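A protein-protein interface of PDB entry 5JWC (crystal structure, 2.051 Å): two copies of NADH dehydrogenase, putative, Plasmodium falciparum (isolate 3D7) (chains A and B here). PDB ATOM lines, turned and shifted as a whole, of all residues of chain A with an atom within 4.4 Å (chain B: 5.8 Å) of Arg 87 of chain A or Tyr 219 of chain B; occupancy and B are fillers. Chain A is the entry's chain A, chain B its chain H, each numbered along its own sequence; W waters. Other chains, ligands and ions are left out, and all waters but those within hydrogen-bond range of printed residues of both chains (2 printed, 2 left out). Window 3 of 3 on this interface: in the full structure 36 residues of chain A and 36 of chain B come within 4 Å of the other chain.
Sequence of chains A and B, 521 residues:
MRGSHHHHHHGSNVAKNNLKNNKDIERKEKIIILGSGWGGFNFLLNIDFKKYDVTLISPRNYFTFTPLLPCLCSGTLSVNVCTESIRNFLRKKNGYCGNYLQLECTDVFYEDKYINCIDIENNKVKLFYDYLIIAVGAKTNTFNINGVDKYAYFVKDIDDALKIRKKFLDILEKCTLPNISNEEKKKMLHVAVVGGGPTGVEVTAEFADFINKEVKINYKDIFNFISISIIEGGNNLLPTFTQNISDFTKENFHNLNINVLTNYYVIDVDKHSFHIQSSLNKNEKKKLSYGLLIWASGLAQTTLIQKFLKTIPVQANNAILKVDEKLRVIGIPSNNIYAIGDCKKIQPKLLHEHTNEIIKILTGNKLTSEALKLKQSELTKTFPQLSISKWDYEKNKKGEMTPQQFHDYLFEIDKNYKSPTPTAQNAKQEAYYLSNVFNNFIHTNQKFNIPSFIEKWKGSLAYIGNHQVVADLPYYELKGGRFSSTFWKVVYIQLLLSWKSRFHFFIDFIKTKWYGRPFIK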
ATOM      1  N   SER A  85      17.492 -18.932 -33.667  1.00  0.00           N
ATOM      2  CA  SER A  85      18.615 -18.731 -32.753  1.00  0.00           C
ATOM      3  C   SER A  85      18.312 -19.345 -31.389  1.00  0.00           C
ATOM      4  O   SER A  85      17.291 -19.042 -30.784  1.00  0.00           O
ATOM      5  CB  SER A  85      18.916 -17.239 -32.588  1.00  0.00           C
ATOM      6  OG  SER A  85      19.549 -16.718 -33.747  1.00  0.00           O
ATOM      7  N   ILE A  86      19.204 -20.191 -30.901  1.00  0.00           N
ATOM      8  CA  ILE A  86      18.974 -20.870 -29.633  1.00  0.00           C
ATOM      9  C   ILE A  86      18.711 -19.894 -28.482  1.00  0.00           C
ATOM     10  O   ILE A  86      17.784 -20.090 -27.695  1.00  0.00           O
ATOM     11  CB  ILE A  86      20.156 -21.754 -29.259  1.00  0.00           C
ATOM     12  CG1 ILE A  86      20.389 -22.812 -30.346  1.00  0.00           C
ATOM     13  CG2 ILE A  86      19.886 -22.443 -27.913  1.00  0.00           C
ATOM     14  CD1 ILE A  86      19.184 -23.689 -30.609  1.00  0.00           C
ATOM     15  N   ARG A  87      19.501 -18.825 -28.398  1.00  0.00           N
ATOM     16  CA  ARG A  87      19.368 -17.910 -27.250  1.00  0.00           C
ATOM     17  C   ARG A  87      18.004 -17.243 -27.152  1.00  0.00           C
ATOM     18  O   ARG A  87      17.616 -16.800 -26.075  1.00  0.00           O
ATOM     19  CB  ARG A  87      20.474 -16.849 -27.265  1.00  0.00           C
ATOM     20  CG  ARG A  87      21.815 -17.468 -27.016  1.00  0.00           C
ATOM     21  CD  ARG A  87      22.899 -16.457 -26.711  1.00  0.00           C
ATOM     22  NE  ARG A  87      24.165 -17.148 -26.489  1.00  0.00           N
ATOM     23  CZ  ARG A  87      24.501 -17.760 -25.350  1.00  0.00           C
ATOM     24  NH1 ARG A  87      23.665 -17.774 -24.305  1.00  0.00           N
ATOM     25  NH2 ARG A  87      25.676 -18.362 -25.251  1.00  0.00           N
ATOM     26  N   ASN A  88      17.255 -17.196 -28.251  1.00  0.00           N
ATOM     27  CA  ASN A  88      15.895 -16.639 -28.207  1.00  0.00           C
ATOM     28  C   ASN A  88      14.915 -17.467 -27.400  1.00  0.00           C
ATOM     29  O   ASN A  88      13.813 -17.008 -27.109  1.00  0.00           O
ATOM     30  CB  ASN A  88      15.314 -16.496 -29.619  1.00  0.00           C
ATOM     31  CG  ASN A  88      15.864 -15.314 -30.362  1.00  0.00           C
ATOM     32  OD1 ASN A  88      16.468 -14.422 -29.768  1.00  0.00           O
ATOM     33  ND2 ASN A  88      15.665 -15.298 -31.679  1.00  0.00           N
ATOM     34  N   PHE A  89      15.290 -18.698 -27.065  1.00  0.00           N
ATOM     35  CA  PHE A  89      14.355 -19.610 -26.409  1.00  0.00           C
ATOM     36  C   PHE A  89      14.869 -20.049 -25.045  1.00  0.00           C
ATOM     37  O   PHE A  89      14.446 -21.080 -24.528  1.00  0.00           O
ATOM     38  CB  PHE A  89      14.097 -20.844 -27.306  1.00  0.00           C
ATOM     39  CG  PHE A  89      13.588 -20.485 -28.676  1.00  0.00           C
ATOM     40  CD1 PHE A  89      12.226 -20.497 -28.953  1.00  0.00           C
ATOM     41  CD2 PHE A  89      14.466 -20.096 -29.666  1.00  0.00           C
ATOM     42  CE1 PHE A  89      11.757 -20.141 -30.219  1.00  0.00           C
ATOM     43  CE2 PHE A  89      14.006 -19.733 -30.940  1.00  0.00           C
ATOM     44  CZ  PHE A  89      12.646 -19.757 -31.213  1.00  0.00           C
ATOM     45  N   LEU A  90      15.797 -19.286 -24.472  1.00  0.00           N
ATOM     46  CA  LEU A  90      16.393 -19.659 -23.188  1.00  0.00           C
ATOM     47  C   LEU A  90      15.670 -19.066 -21.995  1.00  0.00           C
ATOM     48  O   LEU A  90      15.915 -19.475 -20.865  1.00  0.00           O
ATOM     49  CB  LEU A  90      17.870 -19.257 -23.127  1.00  0.00           C
ATOM     50  CG  LEU A  90      18.874 -20.035 -23.977  1.00  0.00           C
ATOM     51  CD1 LEU A  90      20.283 -19.503 -23.783  1.00  0.00           C
ATOM     52  CD2 LEU A  90      18.825 -21.547 -23.659  1.00  0.00           C
ATOM     53  N   ARG A  91      14.785 -18.107 -22.234  1.00  0.00           N
ATOM     54  CA  ARG A  91      14.109 -17.405 -21.140  1.00  0.00           C
ATOM     55  C   ARG A  91      12.608 -17.666 -21.204  1.00  0.00           C
ATOM     56  O   ARG A  91      11.907 -17.057 -21.994  1.00  0.00           O
ATOM     57  CB  ARG A  91      14.404 -15.894 -21.192  1.00  0.00           C
ATOM     58  CG  ARG A  91      15.886 -15.558 -21.038  1.00  0.00           C
ATOM     59  CD  ARG A  91      16.233 -14.122 -21.459  1.00  0.00           C
ATOM     60  NE  ARG A  91      15.828 -13.819 -22.830  1.00  0.00           N
ATOM     61  CZ  ARG A  91      16.526 -14.182 -23.904  1.00  0.00           C
ATOM     62  NH1 ARG A  91      17.650 -14.883 -23.764  1.00  0.00           N
ATOM     63  NH2 ARG A  91      16.096 -13.858 -25.118  1.00  0.00           N
ATOM     64  N   TYR A 100      23.177 -21.759 -22.829  1.00  0.00           N
ATOM     65  CA  TYR A 100      23.721 -22.322 -24.050  1.00  0.00           C
ATOM     66  C   TYR A 100      25.213 -22.024 -24.135  1.00  0.00           C
ATOM     67  O   TYR A 100      25.640 -20.919 -23.839  1.00  0.00           O
ATOM     68  CB  TYR A 100      23.002 -21.775 -25.300  1.00  0.00           C
ATOM     69  CG  TYR A 100      23.801 -22.066 -26.564  1.00  0.00           C
ATOM     70  CD1 TYR A 100      23.877 -23.353 -27.094  1.00  0.00           C
ATOM     71  CD2 TYR A 100      24.541 -21.066 -27.180  1.00  0.00           C
ATOM     72  CE1 TYR A 100      24.640 -23.629 -28.230  1.00  0.00           C
ATOM     73  CE2 TYR A 100      25.298 -21.323 -28.295  1.00  0.00           C
ATOM     74  CZ  TYR A 100      25.353 -22.601 -28.821  1.00  0.00           C
ATOM     75  OH  TYR A 100      26.127 -22.824 -29.946  1.00  0.00           O
ATOM     76  N   LEU B 169      29.297 -10.871 -33.563  1.00  0.00           N
ATOM     77  CA  LEU B 169      28.482 -11.976 -33.066  1.00  0.00           C
ATOM     78  C   LEU B 169      29.370 -13.101 -32.551  1.00  0.00           C
ATOM     79  O   LEU B 169      29.046 -13.714 -31.525  1.00  0.00           O
ATOM     80  CB  LEU B 169      27.531 -12.494 -34.158  1.00  0.00           C
ATOM     81  CG  LEU B 169      26.508 -11.430 -34.576  1.00  0.00           C
ATOM     82  CD1 LEU B 169      25.574 -11.895 -35.710  1.00  0.00           C
ATOM     83  CD2 LEU B 169      25.698 -10.965 -33.357  1.00  0.00           C
ATOM     84  N   LEU B 172      30.752 -12.240 -29.051  1.00  0.00           N
ATOM     85  CA  LEU B 172      29.750 -12.422 -27.998  1.00  0.00           C
ATOM     86  C   LEU B 172      29.681 -13.884 -27.552  1.00  0.00           C
ATOM     87  O   LEU B 172      29.595 -14.181 -26.352  1.00  0.00           O
ATOM     88  CB  LEU B 172      28.362 -11.989 -28.462  1.00  0.00           C
ATOM     89  CG  LEU B 172      28.141 -10.531 -28.856  1.00  0.00           C
ATOM     90  CD1 LEU B 172      26.696 -10.384 -29.363  1.00  0.00           C
ATOM     91  CD2 LEU B 172      28.434  -9.629 -27.653  1.00  0.00           C
ATOM     92  N   GLU B 173      29.688 -14.801 -28.519  1.00  0.00           N
ATOM     93  CA  GLU B 173      29.623 -16.225 -28.167  1.00  0.00           C
ATOM     94  C   GLU B 173      30.900 -16.656 -27.451  1.00  0.00           C
ATOM     95  O   GLU B 173      30.845 -17.372 -26.453  1.00  0.00           O
ATOM     96  CB  GLU B 173      29.382 -17.098 -29.397  1.00  0.00           C
ATOM     97  CG  GLU B 173      27.912 -17.110 -29.865  1.00  0.00           C
ATOM     98  CD  GLU B 173      26.939 -17.634 -28.814  1.00  0.00           C
ATOM     99  OE1 GLU B 173      25.728 -17.300 -28.895  1.00  0.00           O
ATOM    100  OE2 GLU B 173      27.376 -18.375 -27.896  1.00  0.00           O
ATOM    101  N   THR B 176      31.026 -15.839 -23.744  1.00  0.00           N
ATOM    102  CA  THR B 176      30.040 -16.485 -22.893  1.00  0.00           C
ATOM    103  C   THR B 176      30.614 -17.828 -22.367  1.00  0.00           C
ATOM    104  O   THR B 176      30.052 -18.451 -21.469  1.00  0.00           O
ATOM    105  CB  THR B 176      28.698 -16.664 -23.670  1.00  0.00           C
ATOM    106  OG1 THR B 176      28.195 -15.365 -24.046  1.00  0.00           O
ATOM    107  CG2 THR B 176      27.641 -17.339 -22.819  1.00  0.00           C
ATOM    108  N   GLU B 214      18.921  -5.994 -28.302  1.00  0.00           N
ATOM    109  CA  GLU B 214      18.944  -7.448 -28.439  1.00  0.00           C
ATOM    110  C   GLU B 214      20.097  -8.112 -27.700  1.00  0.00           C
ATOM    111  O   GLU B 214      19.929  -9.182 -27.131  1.00  0.00           O
ATOM    112  CB  GLU B 214      18.984  -7.846 -29.915  1.00  0.00           C
ATOM    113  CG  GLU B 214      17.691  -7.522 -30.663  1.00  0.00           C
ATOM    114  CD  GLU B 214      17.674  -6.110 -31.246  1.00  0.00           C
ATOM    115  OE1 GLU B 214      18.605  -5.313 -30.968  1.00  0.00           O
ATOM    116  OE2 GLU B 214      16.713  -5.797 -31.979  1.00  0.00           O
ATOM    117  N   VAL B 215      21.266  -7.490 -27.725  1.00  0.00           N
ATOM    118  CA  VAL B 215      22.429  -8.073 -27.088  1.00  0.00           C
ATOM    119  C   VAL B 215      22.231  -8.088 -25.579  1.00  0.00           C
ATOM    120  O   VAL B 215      22.487  -9.099 -24.921  1.00  0.00           O
ATOM    121  CB  VAL B 215      23.721  -7.317 -27.450  1.00  0.00           C
ATOM    122  CG1 VAL B 215      24.878  -7.820 -26.614  1.00  0.00           C
ATOM    123  CG2 VAL B 215      24.027  -7.476 -28.944  1.00  0.00           C
ATOM    124  N   LYS B 216      21.732  -6.978 -25.046  1.00  0.00           N
ATOM    125  CA  LYS B 216      21.488  -6.875 -23.611  1.00  0.00           C
ATOM    126  C   LYS B 216      20.516  -7.969 -23.143  1.00  0.00           C
ATOM    127  O   LYS B 216      20.703  -8.560 -22.090  1.00  0.00           O
ATOM    128  CB  LYS B 216      20.946  -5.487 -23.251  1.00  0.00           C
ATOM    129  CG  LYS B 216      20.865  -5.221 -21.728  1.00  0.00           C
ATOM    130  CD  LYS B 216      20.213  -3.884 -21.452  1.00  0.00           C
ATOM    131  CE  LYS B 216      20.592  -3.341 -20.071  1.00  0.00           C
ATOM    132  NZ  LYS B 216      19.810  -2.111 -19.751  1.00  0.00           N
ATOM    133  N   ILE B 217      19.512  -8.260 -23.962  1.00  0.00           N
ATOM    134  CA  ILE B 217      18.532  -9.293 -23.648  1.00  0.00           C
ATOM    135  C   ILE B 217      19.104 -10.705 -23.759  1.00  0.00           C
ATOM    136  O   ILE B 217      18.924 -11.508 -22.849  1.00  0.00           O
ATOM    137  CB  ILE B 217      17.299  -9.167 -24.561  1.00  0.00           C
ATOM    138  CG1 ILE B 217      16.511  -7.914 -24.191  1.00  0.00           C
ATOM    139  CG2 ILE B 217      16.405 -10.402 -24.451  1.00  0.00           C
ATOM    140  CD1 ILE B 217      15.441  -7.560 -25.204  1.00  0.00           C
ATOM    141  N   ASN B 218      19.818 -11.002 -24.849  1.00  0.00           N
ATOM    142  CA  ASN B 218      20.317 -12.363 -25.088  1.00  0.00           C
ATOM    143  C   ASN B 218      21.663 -12.712 -24.452  1.00  0.00           C
ATOM    144  O   ASN B 218      22.015 -13.886 -24.343  1.00  0.00           O
ATOM    145  CB  ASN B 218      20.405 -12.616 -26.597  1.00  0.00           C
ATOM    146  CG  ASN B 218      19.048 -12.759 -27.230  1.00  0.00           C
ATOM    147  OD1 ASN B 218      18.505 -13.856 -27.300  1.00  0.00           O
ATOM    148  ND2 ASN B 218      18.481 -11.645 -27.687  1.00  0.00           N
ATOM    149  N   TYR B 219      22.431 -11.702 -24.056  1.00  0.00           N
ATOM    150  CA  TYR B 219      23.744 -11.937 -23.465  1.00  0.00           C
ATOM    151  C   TYR B 219      23.880 -11.127 -22.185  1.00  0.00           C
ATOM    152  O   TYR B 219      24.874 -10.420 -21.978  1.00  0.00           O
ATOM    153  CB  TYR B 219      24.875 -11.580 -24.437  1.00  0.00           C
ATOM    154  CG  TYR B 219      24.904 -12.425 -25.696  1.00  0.00           C
ATOM    155  CD1 TYR B 219      25.726 -13.553 -25.779  1.00  0.00           C
ATOM    156  CD2 TYR B 219      24.116 -12.103 -26.798  1.00  0.00           C
ATOM    157  CE1 TYR B 219      25.763 -14.331 -26.918  1.00  0.00           C
ATOM    158  CE2 TYR B 219      24.148 -12.887 -27.960  1.00  0.00           C
ATOM    159  CZ  TYR B 219      24.975 -13.994 -28.004  1.00  0.00           C
ATOM    160  OH  TYR B 219      25.016 -14.778 -29.129  1.00  0.00           O
ATOM    161  N   LYS B 220      22.879 -11.233 -21.318  1.00  0.00           N
ATOM    162  CA  LYS B 220      22.820 -10.371 -20.134  1.00  0.00           C
ATOM    163  C   LYS B 220      24.084 -10.444 -19.259  1.00  0.00           C
ATOM    164  O   LYS B 220      24.543  -9.424 -18.736  1.00  0.00           O
ATOM    165  CB  LYS B 220      21.581 -10.720 -19.314  1.00  0.00           C
ATOM    166  CG  LYS B 220      21.267  -9.747 -18.194  1.00  0.00           C
ATOM    167  CD  LYS B 220      19.990 -10.170 -17.478  1.00  0.00           C
ATOM    168  CE  LYS B 220      19.737  -9.324 -16.246  1.00  0.00           C
ATOM    169  NZ  LYS B 220      20.798  -9.549 -15.224  1.00  0.00           N
ATOM    170  N   ASP B 221      24.680 -11.625 -19.163  1.00  0.00           N
ATOM    171  CA  ASP B 221      25.833 -11.832 -18.288  1.00  0.00           C
ATOM    172  C   ASP B 221      27.119 -11.132 -18.731  1.00  0.00           C
ATOM    173  O   ASP B 221      28.046 -11.003 -17.937  1.00  0.00           O
ATOM    174  CB  ASP B 221      26.130 -13.329 -18.145  1.00  0.00           C
ATOM    175  CG  ASP B 221      25.171 -14.039 -17.196  1.00  0.00           C
ATOM    176  OD1 ASP B 221      24.616 -13.368 -16.299  1.00  0.00           O
ATOM    177  OD2 ASP B 221      24.985 -15.274 -17.341  1.00  0.00           O
ATOM    178  N   ILE B 222      27.208 -10.719 -19.997  1.00  0.00           N
ATOM    179  CA  ILE B 222      28.418 -10.048 -20.458  1.00  0.00           C
ATOM    180  C   ILE B 222      28.144  -8.627 -20.927  1.00  0.00           C
ATOM    181  O   ILE B 222      29.061  -7.933 -21.353  1.00  0.00           O
ATOM    182  CB  ILE B 222      29.121 -10.822 -21.595  1.00  0.00           C
ATOM    183  CG1 ILE B 222      28.216 -10.951 -22.823  1.00  0.00           C
ATOM    184  CG2 ILE B 222      29.590 -12.184 -21.117  1.00  0.00           C
ATOM    185  CD1 ILE B 222      28.929 -11.601 -23.995  1.00  0.00           C
ATOM    186  N   PHE B 223      26.884  -8.202 -20.848  1.00  0.00           N
ATOM    187  CA  PHE B 223      26.490  -6.886 -21.329  1.00  0.00           C
ATOM    188  C   PHE B 223      27.366  -5.792 -20.747  1.00  0.00           C
ATOM    189  O   PHE B 223      27.855  -4.923 -21.473  1.00  0.00           O
ATOM    190  CB  PHE B 223      25.044  -6.585 -20.978  1.00  0.00           C
ATOM    191  CG  PHE B 223      24.652  -5.160 -21.243  1.00  0.00           C
ATOM    192  CD1 PHE B 223      24.381  -4.736 -22.537  1.00  0.00           C
ATOM    193  CD2 PHE B 223      24.595  -4.231 -20.208  1.00  0.00           C
ATOM    194  CE1 PHE B 223      24.037  -3.420 -22.794  1.00  0.00           C
ATOM    195  CE2 PHE B 223      24.257  -2.910 -20.461  1.00  0.00           C
ATOM    196  CZ  PHE B 223      23.974  -2.508 -21.758  1.00  0.00           C
ATOM    197  N   PHE B 519      20.370 -12.965 -34.953  1.00  0.00           N
ATOM    198  CA  PHE B 519      21.694 -13.364 -34.497  1.00  0.00           C
ATOM    199  C   PHE B 519      22.324 -14.442 -35.384  1.00  0.00           C
ATOM    200  O   PHE B 519      23.450 -14.863 -35.140  1.00  0.00           O
ATOM    201  CB  PHE B 519      21.623 -13.846 -33.044  1.00  0.00           C
ATOM    202  CG  PHE B 519      21.484 -12.726 -32.058  1.00  0.00           C
ATOM    203  CD1 PHE B 519      22.609 -12.166 -31.469  1.00  0.00           C
ATOM    204  CD2 PHE B 519      20.240 -12.209 -31.752  1.00  0.00           C
ATOM    205  CE1 PHE B 519      22.494 -11.113 -30.571  1.00  0.00           C
ATOM    206  CE2 PHE B 519      20.103 -11.149 -30.856  1.00  0.00           C
ATOM    207  CZ  PHE B 519      21.233 -10.598 -30.261  1.00  0.00           C
HETATM  208  O   HOH W   1      21.962 -17.388 -33.573  1.00  0.00           O
HETATM  209  O   HOH W   2      21.840 -16.351 -23.409  1.00  0.00           O
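The side-chain amide oxygen (OD1) of Asn 88 of chain A lies close to the side-chain amide oxygen (OD1) of Asn 218 of chain B (3.2 Å).
The backbone carbonyl oxygen (O) of Arg 87 of chain A sits close to the side-chain amide oxygen (OD1) of Asn 218 of chain B, at 3.3 Å.
OE1 of Glu 173 of chain B lies within salt-bridge range of NE of Arg 87 of chain A, at 2.9 Å.
The guanidinium group (NH2) of Arg 91 of chain A sits at hydrogen-bond distance from the side-chain amide oxygen (OD1) of Asn 218 of chain B, at 3.3 Å.
The backbone carbonyl oxygen (O) of Tyr 100 of chain A is in hydrogen-bond range of the guanidinium group (NH2) of Arg 87 of chain A (2.9 Å).
The guanidinium group of Arg 91 of chain A lies within hydrogen-bond range of the backbone carbonyl oxygen of Arg 87 of chain A, at 3.0 Å.
ND2 of Asn 218 of chain B is in hydrogen-bond range of O of Glu 214 of chain B, at 2.9 Å.
The side-chain carboxylate (OE1) of Glu 173 of chain B sits at hydrogen-bond distance from the side-chain hydroxyl (OH) of Tyr 219 of chain B.
OG1 of Thr 176 of chain B is in hydrogen-bond range of O of Leu 172 of chain B (2.9 Å).
Ser 85 of chain A touches Phe 519 of chain B (OG to CB, 3.6 Å).
Arg 87 of chain A touches Thr 176 of chain B.
Arg 87 of chain A touches Tyr 219 of chain B (NE to CE1, 3.3 Å).
Arg 91 of chain A touches Ile 217 of chain B.
Tyr 100 of chain A touches Glu 173 of chain B (CE2 to OE2, 3.6 Å).
Ile 86 of chain A touches none of the printed residues of chain B.
Arg 87 of chain A touches four residues of chain B.
Of the printed residues of chain B, Asn 88 of chain A touches Asn 218 (3.2 Å).
Of the printed residues of chain B, Arg 91 of chain A touches Ile 217 and Asn 218.
Of the printed residues of chain B, Tyr 100 of chain A touches Glu 173 (3.6 Å).
Of the printed residues of chain A, Glu 173 of chain B touches Arg 87 (2.9 Å) and Tyr 100 (3.6 Å).
Of the printed residues of chain A, Thr 176 of chain B touches Arg 87 (3.3 Å).
The nearest printed residue of chain B that does not touch Arg 87 of chain A is Leu 172 of chain B (5.8 Å).
The nearest printed residue of chain A that does not touch Tyr 219 of chain B is Arg 91 of chain A (5.7 Å).
The nearest printed residue of chain B that does not touch Tyr 100 of chain A is Thr 176 of chain B (4.2 Å).
Hydrophobic or aromatic side chains of chain B that line the printed part of chain A: Ile 217, Tyr 219 and Phe 519.
Printed residues of chain A that touch a printed residue of chain B: Ser 85, Arg 87, Asn 88, Arg 91 and Tyr 100.
Among the printed residues, 9 pairs touch across the chains.
No position is printed for both chains.
Water W2 lies within hydrogen-bond range of NH1 of Arg 87 of chain A (2.5 Å) and O of Asn 218 of chain B (2.6 Å).
Water W1 bridges the side-chain hydroxyl of Ser 85 of chain A (2.5 Å) and the backbone carbonyl oxygen of Phe 519 of chain B (3.3 Å).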
